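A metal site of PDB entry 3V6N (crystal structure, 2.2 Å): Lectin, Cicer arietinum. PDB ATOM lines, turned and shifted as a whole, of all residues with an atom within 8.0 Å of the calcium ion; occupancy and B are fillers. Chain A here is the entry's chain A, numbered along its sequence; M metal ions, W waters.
The calcium ion is bound by O of Asp 174 (2.3 Å), O of Asn 7 (2.4 Å), water W1 (2.4 Å), O of Asp 121 (2.4 Å), O of Asp 65 (2.4 Å), OD1 of Asn 7 (2.5 Å) and water W2 (2.5 Å). The calcium ion has seven donor atoms within binding distance.
N of Asp 174 is in hydrogen-bond range of O of Phe 188 (2.9 Å). The backbone NH (N) of Asn 7 sits at hydrogen-bond distance from the backbone carbonyl oxygen (O) of Phe 21 (2.9 Å). The backbone NH (N) of Asp 121 is in hydrogen-bond range of the backbone carbonyl oxygen (O) of Phe 135. N of Asp 65 lies within hydrogen-bond range of O of Phe 78 (3.0 Å).
Of the 21 residues printed, 4 come within 4 Å of the calcium ion.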
ATOM      1  N   TYR A   5      -2.093  28.202  24.813  1.00  0.00           N
ATOM      2  CA  TYR A   5      -3.107  28.169  25.874  1.00  0.00           C
ATOM      3  C   TYR A   5      -2.990  26.919  26.754  1.00  0.00           C
ATOM      4  O   TYR A   5      -2.073  26.115  26.572  1.00  0.00           O
ATOM      5  CB  TYR A   5      -4.519  28.287  25.270  1.00  0.00           C
ATOM      6  CG  TYR A   5      -4.784  29.648  24.684  1.00  0.00           C
ATOM      7  CD1 TYR A   5      -4.683  29.875  23.322  1.00  0.00           C
ATOM      8  CD2 TYR A   5      -5.101  30.728  25.521  1.00  0.00           C
ATOM      9  CE1 TYR A   5      -4.918  31.131  22.791  1.00  0.00           C
ATOM     10  CE2 TYR A   5      -5.335  31.995  25.000  1.00  0.00           C
ATOM     11  CZ  TYR A   5      -5.248  32.184  23.628  1.00  0.00           C
ATOM     12  OH  TYR A   5      -5.473  33.432  23.103  1.00  0.00           O
ATOM     13  N   ILE A   6      -3.912  26.766  27.701  1.00  0.00           N
ATOM     14  CA  ILE A   6      -3.901  25.600  28.591  1.00  0.00           C
ATOM     15  C   ILE A   6      -4.141  24.297  27.819  1.00  0.00           C
ATOM     16  O   ILE A   6      -5.191  24.085  27.242  1.00  0.00           O
ATOM     17  CB  ILE A   6      -4.927  25.735  29.746  1.00  0.00           C
ATOM     18  CG1 ILE A   6      -4.800  27.117  30.400  1.00  0.00           C
ATOM     19  CG2 ILE A   6      -4.728  24.611  30.761  1.00  0.00           C
ATOM     20  CD1 ILE A   6      -5.805  27.415  31.484  1.00  0.00           C
ATOM     21  N   ASN A   7      -3.139  23.427  27.818  1.00  0.00           N
ATOM     22  CA  ASN A   7      -3.214  22.166  27.102  1.00  0.00           C
ATOM     23  C   ASN A   7      -3.574  20.985  28.028  1.00  0.00           C
ATOM     24  O   ASN A   7      -4.043  19.954  27.558  1.00  0.00           O
ATOM     25  CB  ASN A   7      -1.878  21.914  26.386  1.00  0.00           C
ATOM     26  CG  ASN A   7      -1.980  20.902  25.259  1.00  0.00           C
ATOM     27  OD1 ASN A   7      -3.057  20.414  24.903  1.00  0.00           O
ATOM     28  ND2 ASN A   7      -0.838  20.567  24.678  1.00  0.00           N
ATOM     29  N   ALA A   8      -3.372  21.165  29.333  1.00  0.00           N
ATOM     30  CA  ALA A   8      -3.666  20.122  30.343  1.00  0.00           C
ATOM     31  C   ALA A   8      -3.755  20.711  31.744  1.00  0.00           C
ATOM     32  O   ALA A   8      -3.214  21.790  32.030  1.00  0.00           O
ATOM     33  CB  ALA A   8      -2.645  18.988  30.317  1.00  0.00           C
ATOM     34  N   ALA A   9      -4.410  19.959  32.623  1.00  0.00           N
ATOM     35  CA  ALA A   9      -4.596  20.399  34.000  1.00  0.00           C
ATOM     36  C   ALA A   9      -5.027  19.240  34.861  1.00  0.00           C
ATOM     37  O   ALA A   9      -5.636  18.271  34.377  1.00  0.00           O
ATOM     38  CB  ALA A   9      -5.617  21.528  34.061  1.00  0.00           C
ATOM     39  N   PHE A  21      -0.832  23.270  32.564  1.00  0.00           N
ATOM     40  CA  PHE A  21       0.292  23.029  31.672  1.00  0.00           C
ATOM     41  C   PHE A  21       0.090  23.783  30.386  1.00  0.00           C
ATOM     42  O   PHE A  21      -0.990  23.749  29.792  1.00  0.00           O
ATOM     43  CB  PHE A  21       0.487  21.526  31.448  1.00  0.00           C
ATOM     44  CG  PHE A  21       0.750  20.777  32.730  1.00  0.00           C
ATOM     45  CD1 PHE A  21       2.059  20.635  33.189  1.00  0.00           C
ATOM     46  CD2 PHE A  21      -0.301  20.328  33.513  1.00  0.00           C
ATOM     47  CE1 PHE A  21       2.311  20.013  34.401  1.00  0.00           C
ATOM     48  CE2 PHE A  21      -0.050  19.695  34.715  1.00  0.00           C
ATOM     49  CZ  PHE A  21       1.261  19.534  35.163  1.00  0.00           C
ATOM     50  N   ILE A  64       3.125  18.353  28.672  1.00  0.00           N
ATOM     51  CA  ILE A  64       2.008  17.469  28.992  1.00  0.00           C
ATOM     52  C   ILE A  64       0.740  17.962  28.294  1.00  0.00           C
ATOM     53  O   ILE A  64       0.399  19.164  28.400  1.00  0.00           O
ATOM     54  CB  ILE A  64       1.824  17.390  30.520  1.00  0.00           C
ATOM     55  CG1 ILE A  64       3.024  16.637  31.130  1.00  0.00           C
ATOM     56  CG2 ILE A  64       0.497  16.734  30.909  1.00  0.00           C
ATOM     57  CD1 ILE A  64       3.256  16.848  32.615  1.00  0.00           C
ATOM     58  N   ASP A  65       0.051  17.059  27.577  1.00  0.00           N
ATOM     59  CA  ASP A  65      -1.106  17.475  26.769  1.00  0.00           C
ATOM     60  C   ASP A  65      -2.476  16.961  27.263  1.00  0.00           C
ATOM     61  O   ASP A  65      -3.532  17.328  26.708  1.00  0.00           O
ATOM     62  CB  ASP A  65      -0.871  17.188  25.258  1.00  0.00           C
ATOM     63  CG  ASP A  65      -0.831  15.697  24.941  1.00  0.00           C
ATOM     64  OD1 ASP A  65      -1.240  14.891  25.801  1.00  0.00           O
ATOM     65  OD2 ASP A  65      -0.394  15.343  23.811  1.00  0.00           O
ATOM     66  N   CYS A  66      -2.456  16.139  28.316  1.00  0.00           N
ATOM     67  CA  CYS A  66      -3.648  15.717  29.018  1.00  0.00           C
ATOM     68  C   CYS A  66      -3.245  15.203  30.394  1.00  0.00           C
ATOM     69  O   CYS A  66      -2.151  14.647  30.555  1.00  0.00           O
ATOM     70  CB  CYS A  66      -4.377  14.594  28.248  1.00  0.00           C
ATOM     71  SG  CYS A  66      -5.929  13.996  28.989  1.00  0.00           S
ATOM     72  N   SER A  67      -4.114  15.377  31.383  1.00  0.00           N
ATOM     73  CA  SER A  67      -3.902  14.691  32.677  1.00  0.00           C
ATOM     74  C   SER A  67      -5.094  14.700  33.597  1.00  0.00           C
ATOM     75  O   SER A  67      -6.073  15.439  33.361  1.00  0.00           O
ATOM     76  CB  SER A  67      -2.677  15.220  33.423  1.00  0.00           C
ATOM     77  OG  SER A  67      -2.732  16.596  33.574  1.00  0.00           O
ATOM     78  N   PHE A  78      -0.157  12.677  30.136  1.00  0.00           N
ATOM     79  CA  PHE A  78      -0.054  12.165  28.776  1.00  0.00           C
ATOM     80  C   PHE A  78       0.781  13.085  27.901  1.00  0.00           C
ATOM     81  O   PHE A  78       0.863  14.274  28.157  1.00  0.00           O
ATOM     82  CB  PHE A  78      -1.434  12.040  28.124  1.00  0.00           C
ATOM     83  CG  PHE A  78      -2.367  11.083  28.814  1.00  0.00           C
ATOM     84  CD1 PHE A  78      -2.651   9.861  28.251  1.00  0.00           C
ATOM     85  CD2 PHE A  78      -2.951  11.413  30.041  1.00  0.00           C
ATOM     86  CE1 PHE A  78      -3.519   8.985  28.888  1.00  0.00           C
ATOM     87  CE2 PHE A  78      -3.814  10.550  30.675  1.00  0.00           C
ATOM     88  CZ  PHE A  78      -4.104   9.327  30.103  1.00  0.00           C
ATOM     89  N   ILE A 120      -5.078  11.784  23.884  1.00  0.00           N
ATOM     90  CA  ILE A 120      -6.295  12.264  24.529  1.00  0.00           C
ATOM     91  C   ILE A 120      -6.210  13.787  24.630  1.00  0.00           C
ATOM     92  O   ILE A 120      -5.133  14.320  24.908  1.00  0.00           O
ATOM     93  CB  ILE A 120      -6.484  11.577  25.902  1.00  0.00           C
ATOM     94  CG1 ILE A 120      -6.320  10.058  25.700  1.00  0.00           C
ATOM     95  CG2 ILE A 120      -7.822  11.962  26.530  1.00  0.00           C
ATOM     96  CD1 ILE A 120      -6.495   9.188  26.933  1.00  0.00           C
ATOM     97  N   ASP A 121      -7.328  14.472  24.347  1.00  0.00           N
ATOM     98  CA  ASP A 121      -7.379  15.939  24.423  1.00  0.00           C
ATOM     99  C   ASP A 121      -7.404  16.484  25.861  1.00  0.00           C
ATOM    100  O   ASP A 121      -6.700  17.432  26.180  1.00  0.00           O
ATOM    101  CB  ASP A 121      -8.629  16.476  23.708  1.00  0.00           C
ATOM    102  CG  ASP A 121      -8.562  16.337  22.188  1.00  0.00           C
ATOM    103  OD1 ASP A 121      -7.470  16.199  21.614  1.00  0.00           O
ATOM    104  OD2 ASP A 121      -9.635  16.388  21.555  1.00  0.00           O
ATOM    105  N   ALA A 122      -8.268  15.889  26.699  1.00  0.00           N
ATOM    106  CA  ALA A 122      -8.637  16.458  27.995  1.00  0.00           C
ATOM    107  C   ALA A 122      -9.237  15.368  28.861  1.00  0.00           C
ATOM    108  O   ALA A 122      -9.746  14.358  28.353  1.00  0.00           O
ATOM    109  CB  ALA A 122      -9.634  17.610  27.824  1.00  0.00           C
ATOM    110  N   ALA A 123      -9.161  15.556  30.185  1.00  0.00           N
ATOM    111  CA  ALA A 123      -9.686  14.566  31.120  1.00  0.00           C
ATOM    112  C   ALA A 123      -9.981  15.230  32.441  1.00  0.00           C
ATOM    113  O   ALA A 123      -9.305  16.189  32.824  1.00  0.00           O
ATOM    114  CB  ALA A 123      -8.682  13.447  31.307  1.00  0.00           C
ATOM    115  N   PHE A 135     -11.694  12.937  26.947  1.00  0.00           N
ATOM    116  CA  PHE A 135     -12.245  13.589  25.755  1.00  0.00           C
ATOM    117  C   PHE A 135     -11.283  13.505  24.587  1.00  0.00           C
ATOM    118  O   PHE A 135     -10.080  13.791  24.757  1.00  0.00           O
ATOM    119  CB  PHE A 135     -12.594  15.069  26.045  1.00  0.00           C
ATOM    120  CG  PHE A 135     -13.591  15.257  27.150  1.00  0.00           C
ATOM    121  CD1 PHE A 135     -14.953  15.271  26.874  1.00  0.00           C
ATOM    122  CD2 PHE A 135     -13.175  15.418  28.476  1.00  0.00           C
ATOM    123  CE1 PHE A 135     -15.888  15.433  27.895  1.00  0.00           C
ATOM    124  CE2 PHE A 135     -14.107  15.594  29.492  1.00  0.00           C
ATOM    125  CZ  PHE A 135     -15.470  15.597  29.207  1.00  0.00           C
ATOM    126  N   MET A 173     -12.535  19.826  23.567  1.00  0.00           N
ATOM    127  CA  MET A 173     -11.986  20.514  24.713  1.00  0.00           C
ATOM    128  C   MET A 173     -10.467  20.359  24.703  1.00  0.00           C
ATOM    129  O   MET A 173      -9.970  19.301  24.322  1.00  0.00           O
ATOM    130  CB  MET A 173     -12.578  19.950  25.993  1.00  0.00           C
ATOM    131  CG  MET A 173     -14.052  20.288  26.093  1.00  0.00           C
ATOM    132  SD  MET A 173     -15.030  18.932  26.734  1.00  0.00           S
ATOM    133  CE  MET A 173     -16.661  19.482  26.213  1.00  0.00           C
ATOM    134  N   ASP A 174      -9.748  21.416  25.070  1.00  0.00           N
ATOM    135  CA  ASP A 174      -8.289  21.420  25.006  1.00  0.00           C
ATOM    136  C   ASP A 174      -7.725  20.876  26.318  1.00  0.00           C
ATOM    137  O   ASP A 174      -6.668  20.248  26.334  1.00  0.00           O
ATOM    138  CB  ASP A 174      -7.756  22.858  24.783  1.00  0.00           C
ATOM    139  CG  ASP A 174      -7.881  23.339  23.340  1.00  0.00           C
ATOM    140  OD1 ASP A 174      -8.287  22.517  22.479  1.00  0.00           O
ATOM    141  OD2 ASP A 174      -7.576  24.533  23.045  1.00  0.00           O
ATOM    142  N   SER A 175      -8.469  21.091  27.401  1.00  0.00           N
ATOM    143  CA  SER A 175      -8.008  20.869  28.761  1.00  0.00           C
ATOM    144  C   SER A 175      -9.166  20.927  29.747  1.00  0.00           C
ATOM    145  O   SER A 175     -10.184  21.547  29.457  1.00  0.00           O
ATOM    146  CB  SER A 175      -6.983  21.954  29.106  1.00  0.00           C
ATOM    147  OG  SER A 175      -6.540  21.789  30.410  1.00  0.00           O
ATOM    148  N   ALA A 176      -9.012  20.292  30.905  1.00  0.00           N
ATOM    149  CA  ALA A 176     -10.026  20.258  31.966  1.00  0.00           C
ATOM    150  C   ALA A 176      -9.458  19.884  33.338  1.00  0.00           C
ATOM    151  O   ALA A 176      -8.427  19.178  33.428  1.00  0.00           O
ATOM    152  CB  ALA A 176     -11.146  19.290  31.595  1.00  0.00           C
ATOM    153  N   PHE A 188     -11.619  23.975  29.277  1.00  0.00           N
ATOM    154  CA  PHE A 188     -10.876  25.053  28.621  1.00  0.00           C
ATOM    155  C   PHE A 188     -10.807  24.847  27.109  1.00  0.00           C
ATOM    156  O   PHE A 188     -10.699  23.708  26.630  1.00  0.00           O
ATOM    157  CB  PHE A 188      -9.463  25.168  29.217  1.00  0.00           C
ATOM    158  CG  PHE A 188      -9.457  25.432  30.708  1.00  0.00           C
ATOM    159  CD1 PHE A 188      -9.331  24.382  31.604  1.00  0.00           C
ATOM    160  CD2 PHE A 188      -9.601  26.729  31.202  1.00  0.00           C
ATOM    161  CE1 PHE A 188      -9.337  24.625  32.987  1.00  0.00           C
ATOM    162  CE2 PHE A 188      -9.622  26.978  32.569  1.00  0.00           C
ATOM    163  CZ  PHE A 188      -9.492  25.919  33.463  1.00  0.00           C
HETATM  164 CA    CA M   1      -4.936  18.910  25.640  1.00  0.00          CA
HETATM  165  O   HOH W   1      -5.762  19.537  23.516  1.00  0.00           O
HETATM  166  O   HOH W   2      -4.103  17.094  24.092  1.00  0.00           O
